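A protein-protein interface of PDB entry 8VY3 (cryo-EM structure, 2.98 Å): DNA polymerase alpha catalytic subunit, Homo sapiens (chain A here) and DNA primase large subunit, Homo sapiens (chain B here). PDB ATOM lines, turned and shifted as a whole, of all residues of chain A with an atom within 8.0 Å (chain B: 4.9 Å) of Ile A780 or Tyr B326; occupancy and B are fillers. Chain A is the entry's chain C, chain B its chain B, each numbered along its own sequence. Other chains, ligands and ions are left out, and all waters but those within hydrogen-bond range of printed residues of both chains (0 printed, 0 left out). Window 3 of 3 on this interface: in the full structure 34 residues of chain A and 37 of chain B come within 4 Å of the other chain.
Printed residues of chain B that touch a printed residue of chain A: Lys B322, Gly B323 and Tyr B326.
Hydrophobic or aromatic side chains of chain B within 4 Å of the printed part of chain A: Tyr B326.
Ser B325 touches none of the printed residues of chain A.
Of the printed residues of chain B, Thr A900 touches Tyr B326 (3.7 Å).
Printed residues of chain A within 4 Å of Lys B322: Gln A776.
Printed residues of chain B within 4 Å of Gln A776: Lys B322, Gly B323 and Tyr B326.
Printed residues of chain A within 4 Å of Gly B323: Gln A776 (3.5 Å).
The nearest printed residue of chain B that does not touch Ile A780 is Lys B322 (4.9 Å).
Among the printed residues, merely in contact across the chains: Gln A776 with Gly B323 (3.5 Å), Gln A776 with Tyr B326 (3.5 Å), Ile A780 with Tyr B326 (3.5 Å) and Thr A900 with Tyr B326 (3.7 Å).
The side-chain amide nitrogen (NE2) of Gln A776 lies within hydrogen-bond range of the backbone carbonyl oxygen (O) of Lys B322, at 3.0 Å.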
ATOM      1  N   GLU A 773      -2.297 -17.247 -18.546  1.00  0.00           N
ATOM      2  CA  GLU A 773      -3.581 -17.849 -18.886  1.00  0.00           C
ATOM      3  C   GLU A 773      -3.918 -17.634 -20.358  1.00  0.00           C
ATOM      4  O   GLU A 773      -4.437 -18.534 -21.027  1.00  0.00           O
ATOM      5  CB  GLU A 773      -4.676 -17.278 -17.984  1.00  0.00           C
ATOM      6  CG  GLU A 773      -6.029 -17.126 -18.652  1.00  0.00           C
ATOM      7  CD  GLU A 773      -7.036 -16.422 -17.768  1.00  0.00           C
ATOM      8  OE1 GLU A 773      -6.827 -16.386 -16.537  1.00  0.00           O
ATOM      9  OE2 GLU A 773      -8.038 -15.903 -18.303  1.00  0.00           O
ATOM     10  N   ASN A 774      -3.632 -16.439 -20.878  1.00  0.00           N
ATOM     11  CA  ASN A 774      -3.898 -16.153 -22.284  1.00  0.00           C
ATOM     12  C   ASN A 774      -2.957 -16.931 -23.194  1.00  0.00           C
ATOM     13  O   ASN A 774      -3.365 -17.430 -24.249  1.00  0.00           O
ATOM     14  CB  ASN A 774      -3.773 -14.653 -22.545  1.00  0.00           C
ATOM     15  CG  ASN A 774      -4.997 -13.883 -22.107  1.00  0.00           C
ATOM     16  OD1 ASN A 774      -5.048 -12.661 -22.224  1.00  0.00           O
ATOM     17  ND2 ASN A 774      -5.992 -14.595 -21.595  1.00  0.00           N
ATOM     18  N   ILE A 775      -1.684 -17.029 -22.810  1.00  0.00           N
ATOM     19  CA  ILE A 775      -0.712 -17.774 -23.606  1.00  0.00           C
ATOM     20  C   ILE A 775      -1.041 -19.260 -23.594  1.00  0.00           C
ATOM     21  O   ILE A 775      -0.999 -19.929 -24.632  1.00  0.00           O
ATOM     22  CB  ILE A 775       0.713 -17.502 -23.092  1.00  0.00           C
ATOM     23  CG1 ILE A 775       1.198 -16.132 -23.567  1.00  0.00           C
ATOM     24  CG2 ILE A 775       1.666 -18.593 -23.543  1.00  0.00           C
ATOM     25  CD1 ILE A 775       2.638 -15.844 -23.235  1.00  0.00           C
ATOM     26  N   GLN A 776      -1.383 -19.796 -22.422  1.00  0.00           N
ATOM     27  CA  GLN A 776      -1.711 -21.214 -22.305  1.00  0.00           C
ATOM     28  C   GLN A 776      -2.944 -21.563 -23.128  1.00  0.00           C
ATOM     29  O   GLN A 776      -2.998 -22.610 -23.781  1.00  0.00           O
ATOM     30  CB  GLN A 776      -1.924 -21.572 -20.835  1.00  0.00           C
ATOM     31  CG  GLN A 776      -2.780 -22.800 -20.608  1.00  0.00           C
ATOM     32  CD  GLN A 776      -2.609 -23.379 -19.221  1.00  0.00           C
ATOM     33  OE1 GLN A 776      -1.992 -22.764 -18.352  1.00  0.00           O
ATOM     34  NE2 GLN A 776      -3.156 -24.567 -19.005  1.00  0.00           N
ATOM     35  N   LYS A 777      -3.949 -20.691 -23.105  1.00  0.00           N
ATOM     36  CA  LYS A 777      -5.208 -20.930 -23.800  1.00  0.00           C
ATOM     37  C   LYS A 777      -5.014 -21.032 -25.307  1.00  0.00           C
ATOM     38  O   LYS A 777      -5.613 -21.893 -25.956  1.00  0.00           O
ATOM     39  CB  LYS A 777      -6.201 -19.815 -23.473  1.00  0.00           C
ATOM     40  CG  LYS A 777      -7.604 -20.039 -23.999  1.00  0.00           C
ATOM     41  CD  LYS A 777      -8.418 -18.761 -23.906  1.00  0.00           C
ATOM     42  CE  LYS A 777      -8.322 -18.149 -22.517  1.00  0.00           C
ATOM     43  NZ  LYS A 777      -8.729 -16.718 -22.505  1.00  0.00           N
ATOM     44  N   ARG A 778      -4.190 -20.152 -25.874  1.00  0.00           N
ATOM     45  CA  ARG A 778      -3.925 -20.153 -27.308  1.00  0.00           C
ATOM     46  C   ARG A 778      -3.152 -21.396 -27.727  1.00  0.00           C
ATOM     47  O   ARG A 778      -3.454 -22.006 -28.756  1.00  0.00           O
ATOM     48  CB  ARG A 778      -3.155 -18.893 -27.706  1.00  0.00           C
ATOM     49  CG  ARG A 778      -2.522 -18.946 -29.087  1.00  0.00           C
ATOM     50  CD  ARG A 778      -3.565 -19.094 -30.178  1.00  0.00           C
ATOM     51  NE  ARG A 778      -4.153 -17.814 -30.549  1.00  0.00           N
ATOM     52  CZ  ARG A 778      -3.692 -17.033 -31.517  1.00  0.00           C
ATOM     53  NH1 ARG A 778      -2.636 -17.374 -32.236  1.00  0.00           N
ATOM     54  NH2 ARG A 778      -4.305 -15.879 -31.768  1.00  0.00           N
ATOM     55  N   LEU A 779      -2.151 -21.778 -26.934  1.00  0.00           N
ATOM     56  CA  LEU A 779      -1.305 -22.914 -27.274  1.00  0.00           C
ATOM     57  C   LEU A 779      -2.072 -24.229 -27.209  1.00  0.00           C
ATOM     58  O   LEU A 779      -1.781 -25.172 -27.951  1.00  0.00           O
ATOM     59  CB  LEU A 779      -0.091 -22.942 -26.341  1.00  0.00           C
ATOM     60  CG  LEU A 779       1.244 -22.564 -26.978  1.00  0.00           C
ATOM     61  CD1 LEU A 779       1.254 -21.094 -27.335  1.00  0.00           C
ATOM     62  CD2 LEU A 779       2.376 -22.885 -26.030  1.00  0.00           C
ATOM     63  N   ILE A 780      -3.049 -24.313 -26.308  1.00  0.00           N
ATOM     64  CA  ILE A 780      -3.906 -25.488 -26.191  1.00  0.00           C
ATOM     65  C   ILE A 780      -4.708 -25.649 -27.476  1.00  0.00           C
ATOM     66  O   ILE A 780      -4.824 -26.754 -28.016  1.00  0.00           O
ATOM     67  CB  ILE A 780      -4.841 -25.379 -24.972  1.00  0.00           C
ATOM     68  CG1 ILE A 780      -4.062 -25.592 -23.672  1.00  0.00           C
ATOM     69  CG2 ILE A 780      -5.985 -26.370 -25.084  1.00  0.00           C
ATOM     70  CD1 ILE A 780      -3.978 -27.029 -23.229  1.00  0.00           C
ATOM     71  N   GLU A 781      -5.260 -24.542 -27.972  1.00  0.00           N
ATOM     72  CA  GLU A 781      -6.088 -24.586 -29.173  1.00  0.00           C
ATOM     73  C   GLU A 781      -5.269 -24.962 -30.403  1.00  0.00           C
ATOM     74  O   GLU A 781      -5.737 -25.714 -31.264  1.00  0.00           O
ATOM     75  CB  GLU A 781      -6.780 -23.237 -29.370  1.00  0.00           C
ATOM     76  CG  GLU A 781      -6.888 -22.784 -30.814  1.00  0.00           C
ATOM     77  CD  GLU A 781      -7.473 -21.393 -30.942  1.00  0.00           C
ATOM     78  OE1 GLU A 781      -7.131 -20.691 -31.917  1.00  0.00           O
ATOM     79  OE2 GLU A 781      -8.271 -20.999 -30.066  1.00  0.00           O
ATOM     80  N   ILE A 782      -4.044 -24.446 -30.502  1.00  0.00           N
ATOM     81  CA  ILE A 782      -3.191 -24.657 -31.669  1.00  0.00           C
ATOM     82  C   ILE A 782      -2.892 -26.141 -31.838  1.00  0.00           C
ATOM     83  O   ILE A 782      -2.957 -26.674 -32.951  1.00  0.00           O
ATOM     84  CB  ILE A 782      -1.892 -23.839 -31.556  1.00  0.00           C
ATOM     85  CG1 ILE A 782      -2.122 -22.417 -32.061  1.00  0.00           C
ATOM     86  CG2 ILE A 782      -0.767 -24.497 -32.337  1.00  0.00           C
ATOM     87  CD1 ILE A 782      -0.855 -21.625 -32.235  1.00  0.00           C
ATOM     88  N   GLY A 783      -2.567 -26.816 -30.739  1.00  0.00           N
ATOM     89  CA  GLY A 783      -2.319 -28.243 -30.776  1.00  0.00           C
ATOM     90  C   GLY A 783      -3.524 -29.030 -31.246  1.00  0.00           C
ATOM     91  O   GLY A 783      -3.388 -29.995 -32.002  1.00  0.00           O
ATOM     92  N   GLU A 784      -4.711 -28.627 -30.795  1.00  0.00           N
ATOM     93  CA  GLU A 784      -5.959 -29.261 -31.206  1.00  0.00           C
ATOM     94  C   GLU A 784      -6.221 -29.056 -32.692  1.00  0.00           C
ATOM     95  O   GLU A 784      -6.653 -29.980 -33.386  1.00  0.00           O
ATOM     96  CB  GLU A 784      -7.128 -28.707 -30.392  1.00  0.00           C
ATOM     97  CG  GLU A 784      -7.215 -29.237 -28.975  1.00  0.00           C
ATOM     98  CD  GLU A 784      -8.202 -28.458 -28.129  1.00  0.00           C
ATOM     99  OE1 GLU A 784      -8.038 -28.430 -26.892  1.00  0.00           O
ATOM    100  OE2 GLU A 784      -9.138 -27.866 -28.705  1.00  0.00           O
ATOM    101  N   ASN A 785      -5.970 -27.840 -33.182  1.00  0.00           N
ATOM    102  CA  ASN A 785      -6.265 -27.512 -34.573  1.00  0.00           C
ATOM    103  C   ASN A 785      -5.399 -28.320 -35.534  1.00  0.00           C
ATOM    104  O   ASN A 785      -5.871 -28.777 -36.580  1.00  0.00           O
ATOM    105  CB  ASN A 785      -6.068 -26.015 -34.804  1.00  0.00           C
ATOM    106  CG  ASN A 785      -7.323 -25.217 -34.541  1.00  0.00           C
ATOM    107  OD1 ASN A 785      -7.558 -24.183 -35.166  1.00  0.00           O
ATOM    108  ND2 ASN A 785      -8.140 -25.693 -33.609  1.00  0.00           N
ATOM    109  N   VAL A 786      -4.123 -28.492 -35.197  1.00  0.00           N
ATOM    110  CA  VAL A 786      -3.171 -29.187 -36.058  1.00  0.00           C
ATOM    111  C   VAL A 786      -3.579 -30.646 -36.213  1.00  0.00           C
ATOM    112  O   VAL A 786      -3.539 -31.199 -37.318  1.00  0.00           O
ATOM    113  CB  VAL A 786      -1.739 -29.065 -35.503  1.00  0.00           C
ATOM    114  CG1 VAL A 786      -0.793 -29.979 -36.255  1.00  0.00           C
ATOM    115  CG2 VAL A 786      -1.264 -27.626 -35.589  1.00  0.00           C
ATOM    116  N   LEU A 897       6.447 -28.308 -19.851  1.00  0.00           N
ATOM    117  CA  LEU A 897       5.065 -27.861 -19.694  1.00  0.00           C
ATOM    118  C   LEU A 897       4.464 -27.375 -21.009  1.00  0.00           C
ATOM    119  O   LEU A 897       3.282 -27.605 -21.282  1.00  0.00           O
ATOM    120  CB  LEU A 897       4.990 -26.762 -18.630  1.00  0.00           C
ATOM    121  CG  LEU A 897       3.622 -26.490 -18.001  1.00  0.00           C
ATOM    122  CD1 LEU A 897       2.850 -27.778 -17.787  1.00  0.00           C
ATOM    123  CD2 LEU A 897       3.780 -25.740 -16.695  1.00  0.00           C
ATOM    124  N   ILE A 898       5.258 -26.687 -21.836  1.00  0.00           N
ATOM    125  CA  ILE A 898       4.764 -26.248 -23.142  1.00  0.00           C
ATOM    126  C   ILE A 898       4.387 -27.456 -23.991  1.00  0.00           C
ATOM    127  O   ILE A 898       3.367 -27.458 -24.687  1.00  0.00           O
ATOM    128  CB  ILE A 898       5.803 -25.366 -23.858  1.00  0.00           C
ATOM    129  CG1 ILE A 898       5.905 -23.986 -23.210  1.00  0.00           C
ATOM    130  CG2 ILE A 898       5.448 -25.200 -25.322  1.00  0.00           C
ATOM    131  CD1 ILE A 898       7.031 -23.856 -22.234  1.00  0.00           C
ATOM    132  N   ALA A 899       5.209 -28.504 -23.938  1.00  0.00           N
ATOM    133  CA  ALA A 899       4.967 -29.725 -24.694  1.00  0.00           C
ATOM    134  C   ALA A 899       3.662 -30.385 -24.271  1.00  0.00           C
ATOM    135  O   ALA A 899       2.924 -30.907 -25.111  1.00  0.00           O
ATOM    136  CB  ALA A 899       6.131 -30.699 -24.520  1.00  0.00           C
ATOM    137  N   THR A 900       3.376 -30.375 -22.968  1.00  0.00           N
ATOM    138  CA  THR A 900       2.132 -30.950 -22.467  1.00  0.00           C
ATOM    139  C   THR A 900       0.915 -30.205 -23.005  1.00  0.00           C
ATOM    140  O   THR A 900      -0.100 -30.829 -23.334  1.00  0.00           O
ATOM    141  CB  THR A 900       2.132 -30.941 -20.940  1.00  0.00           C
ATOM    142  OG1 THR A 900       3.219 -31.740 -20.459  1.00  0.00           O
ATOM    143  CG2 THR A 900       0.831 -31.505 -20.402  1.00  0.00           C
ATOM    144  N   TRP A 901       0.999 -28.875 -23.105  1.00  0.00           N
ATOM    145  CA  TRP A 901      -0.110 -28.100 -23.649  1.00  0.00           C
ATOM    146  C   TRP A 901      -0.381 -28.453 -25.102  1.00  0.00           C
ATOM    147  O   TRP A 901      -1.505 -28.285 -25.586  1.00  0.00           O
ATOM    148  CB  TRP A 901       0.181 -26.603 -23.547  1.00  0.00           C
ATOM    149  CG  TRP A 901       0.293 -26.076 -22.155  1.00  0.00           C
ATOM    150  CD1 TRP A 901      -0.209 -26.637 -21.023  1.00  0.00           C
ATOM    151  CD2 TRP A 901       0.936 -24.862 -21.753  1.00  0.00           C
ATOM    152  NE1 TRP A 901       0.093 -25.858 -19.935  1.00  0.00           N
ATOM    153  CE2 TRP A 901       0.796 -24.759 -20.358  1.00  0.00           C
ATOM    154  CE3 TRP A 901       1.622 -23.855 -22.437  1.00  0.00           C
ATOM    155  CZ2 TRP A 901       1.314 -23.692 -19.634  1.00  0.00           C
ATOM    156  CZ3 TRP A 901       2.137 -22.796 -21.716  1.00  0.00           C
ATOM    157  CH2 TRP A 901       1.979 -22.722 -20.331  1.00  0.00           C
ATOM    158  N   LEU A 902       0.632 -28.942 -25.812  1.00  0.00           N
ATOM    159  CA  LEU A 902       0.561 -29.110 -27.255  1.00  0.00           C
ATOM    160  C   LEU A 902       0.153 -30.514 -27.685  1.00  0.00           C
ATOM    161  O   LEU A 902      -0.271 -30.689 -28.831  1.00  0.00           O
ATOM    162  CB  LEU A 902       1.914 -28.760 -27.879  1.00  0.00           C
ATOM    163  CG  LEU A 902       2.171 -27.282 -28.178  1.00  0.00           C
ATOM    164  CD1 LEU A 902       3.652 -27.035 -28.377  1.00  0.00           C
ATOM    165  CD2 LEU A 902       1.388 -26.829 -29.389  1.00  0.00           C
ATOM    166  N   GLY A 903       0.263 -31.507 -26.811  1.00  0.00           N
ATOM    167  CA  GLY A 903      -0.082 -32.861 -27.189  1.00  0.00           C
ATOM    168  C   GLY A 903       0.355 -33.852 -26.128  1.00  0.00           C
ATOM    169  O   GLY A 903       0.383 -33.545 -24.934  1.00  0.00           O
ATOM    170  N   ASP B 321     -10.027 -27.099 -14.924  1.00  0.00           N
ATOM    171  CA  ASP B 321      -9.412 -28.250 -15.574  1.00  0.00           C
ATOM    172  C   ASP B 321      -8.586 -27.826 -16.782  1.00  0.00           C
ATOM    173  O   ASP B 321      -7.581 -28.459 -17.120  1.00  0.00           O
ATOM    174  CB  ASP B 321     -10.486 -29.260 -15.991  1.00  0.00           C
ATOM    175  CG  ASP B 321     -11.602 -29.376 -14.979  1.00  0.00           C
ATOM    176  OD1 ASP B 321     -12.721 -28.908 -15.271  1.00  0.00           O
ATOM    177  OD2 ASP B 321     -11.366 -29.944 -13.892  1.00  0.00           O
ATOM    178  N   LYS B 322      -9.010 -26.753 -17.452  1.00  0.00           N
ATOM    179  CA  LYS B 322      -8.276 -26.294 -18.625  1.00  0.00           C
ATOM    180  C   LYS B 322      -6.994 -25.560 -18.251  1.00  0.00           C
ATOM    181  O   LYS B 322      -6.003 -25.636 -18.984  1.00  0.00           O
ATOM    182  CB  LYS B 322      -9.165 -25.395 -19.483  1.00  0.00           C
ATOM    183  CG  LYS B 322     -10.011 -26.149 -20.496  1.00  0.00           C
ATOM    184  CD  LYS B 322     -11.125 -25.275 -21.045  1.00  0.00           C
ATOM    185  CE  LYS B 322     -11.947 -26.022 -22.081  1.00  0.00           C
ATOM    186  NZ  LYS B 322     -11.184 -26.248 -23.338  1.00  0.00           N
ATOM    187  N   GLY B 323      -6.987 -24.842 -17.130  1.00  0.00           N
ATOM    188  CA  GLY B 323      -5.865 -23.970 -16.842  1.00  0.00           C
ATOM    189  C   GLY B 323      -5.030 -24.255 -15.609  1.00  0.00           C
ATOM    190  O   GLY B 323      -3.823 -23.997 -15.616  1.00  0.00           O
ATOM    191  N   TYR B 324      -5.634 -24.783 -14.548  1.00  0.00           N
ATOM    192  CA  TYR B 324      -4.935 -24.938 -13.275  1.00  0.00           C
ATOM    193  C   TYR B 324      -4.616 -26.377 -12.912  1.00  0.00           C
ATOM    194  O   TYR B 324      -3.771 -26.610 -12.049  1.00  0.00           O
ATOM    195  CB  TYR B 324      -5.753 -24.308 -12.141  1.00  0.00           C
ATOM    196  CG  TYR B 324      -5.569 -22.814 -12.010  1.00  0.00           C
ATOM    197  CD1 TYR B 324      -4.666 -22.132 -12.813  1.00  0.00           C
ATOM    198  CD2 TYR B 324      -6.303 -22.083 -11.086  1.00  0.00           C
ATOM    199  CE1 TYR B 324      -4.496 -20.766 -12.697  1.00  0.00           C
ATOM    200  CE2 TYR B 324      -6.140 -20.717 -10.967  1.00  0.00           C
ATOM    201  CZ  TYR B 324      -5.236 -20.064 -11.773  1.00  0.00           C
ATOM    202  OH  TYR B 324      -5.071 -18.703 -11.656  1.00  0.00           O
ATOM    203  N   SER B 325      -5.271 -27.354 -13.537  1.00  0.00           N
ATOM    204  CA  SER B 325      -4.972 -28.749 -13.236  1.00  0.00           C
ATOM    205  C   SER B 325      -3.597 -29.141 -13.761  1.00  0.00           C
ATOM    206  O   SER B 325      -2.930 -30.018 -13.203  1.00  0.00           O
ATOM    207  CB  SER B 325      -6.057 -29.653 -13.824  1.00  0.00           C
ATOM    208  OG  SER B 325      -5.632 -30.230 -15.045  1.00  0.00           O
ATOM    209  N   TYR B 326      -3.159 -28.495 -14.843  1.00  0.00           N
ATOM    210  CA  TYR B 326      -1.873 -28.792 -15.461  1.00  0.00           C
ATOM    211  C   TYR B 326      -0.718 -28.550 -14.499  1.00  0.00           C
ATOM    212  O   TYR B 326       0.179 -29.387 -14.381  1.00  0.00           O
ATOM    213  CB  TYR B 326      -1.682 -27.947 -16.722  1.00  0.00           C
ATOM    214  CG  TYR B 326      -2.394 -28.478 -17.947  1.00  0.00           C
ATOM    215  CD1 TYR B 326      -3.603 -27.938 -18.359  1.00  0.00           C
ATOM    216  CD2 TYR B 326      -1.845 -29.504 -18.700  1.00  0.00           C
ATOM    217  CE1 TYR B 326      -4.252 -28.416 -19.478  1.00  0.00           C
ATOM    218  CE2 TYR B 326      -2.488 -29.986 -19.822  1.00  0.00           C
ATOM    219  CZ  TYR B 326      -3.690 -29.438 -20.205  1.00  0.00           C
ATOM    220  OH  TYR B 326      -4.333 -29.917 -21.322  1.00  0.00           O
ATOM    221  N   ASN B 327      -0.735 -27.410 -13.805  1.00  0.00           N
ATOM    222  CA  ASN B 327       0.358 -27.072 -12.898  1.00  0.00           C
ATOM    223  C   ASN B 327       0.402 -28.015 -11.701  1.00  0.00           C
ATOM    224  O   ASN B 327       1.475 -28.462 -11.284  1.00  0.00           O
ATOM    225  CB  ASN B 327       0.221 -25.622 -12.438  1.00  0.00           C
ATOM    226  CG  ASN B 327       0.668 -24.636 -13.495  1.00  0.00           C
ATOM    227  OD1 ASN B 327       0.075 -24.549 -14.570  1.00  0.00           O
ATOM    228  ND2 ASN B 327       1.725 -23.891 -13.199  1.00  0.00           N
ATOM    229  N   ILE B 328      -0.767 -28.330 -11.137  1.00  0.00           N
ATOM    230  CA  ILE B 328      -0.826 -29.256 -10.011  1.00  0.00           C
ATOM    231  C   ILE B 328      -0.338 -30.637 -10.426  1.00  0.00           C
ATOM    232  O   ILE B 328       0.407 -31.290  -9.687  1.00  0.00           O
ATOM    233  CB  ILE B 328      -2.260 -29.308  -9.447  1.00  0.00           C
ATOM    234  CG1 ILE B 328      -2.555 -28.060  -8.621  1.00  0.00           C
ATOM    235  CG2 ILE B 328      -2.457 -30.546  -8.592  1.00  0.00           C
ATOM    236  CD1 ILE B 328      -3.993 -27.953  -8.187  1.00  0.00           C
ATOM    237  N   ARG B 329      -0.745 -31.103 -11.610  1.00  0.00           N
ATOM    238  CA  ARG B 329      -0.291 -32.404 -12.091  1.00  0.00           C
ATOM    239  C   ARG B 329       1.210 -32.407 -12.354  1.00  0.00           C
ATOM    240  O   ARG B 329       1.888 -33.406 -12.092  1.00  0.00           O
ATOM    241  CB  ARG B 329      -1.064 -32.787 -13.352  1.00  0.00           C
ATOM    242  CG  ARG B 329      -1.829 -34.089 -13.234  1.00  0.00           C
ATOM    243  CD  ARG B 329      -3.198 -33.984 -13.883  1.00  0.00           C
ATOM    244  NE  ARG B 329      -3.104 -33.567 -15.275  1.00  0.00           N
ATOM    245  CZ  ARG B 329      -4.055 -32.908 -15.924  1.00  0.00           C
ATOM    246  NH1 ARG B 329      -5.192 -32.580 -15.337  1.00  0.00           N
ATOM    247  NH2 ARG B 329      -3.858 -32.572 -17.196  1.00  0.00           N
ATOM    248  N   HIS B 330       1.744 -31.305 -12.881  1.00  0.00           N
ATOM    249  CA  HIS B 330       3.173 -31.167 -13.138  1.00  0.00           C
ATOM    250  C   HIS B 330       3.976 -31.190 -11.844  1.00  0.00           C
ATOM    251  O   HIS B 330       5.071 -31.755 -11.797  1.00  0.00           O
ATOM    252  CB  HIS B 330       3.444 -29.868 -13.900  1.00  0.00           C
ATOM    253  CG  HIS B 330       4.792 -29.812 -14.548  1.00  0.00           C
ATOM    254  ND1 HIS B 330       5.205 -30.728 -15.489  1.00  0.00           N
ATOM    255  CD2 HIS B 330       5.817 -28.940 -14.396  1.00  0.00           C
ATOM    256  CE1 HIS B 330       6.429 -30.427 -15.887  1.00  0.00           C
ATOM    257  NE2 HIS B 330       6.823 -29.345 -15.239  1.00  0.00           N
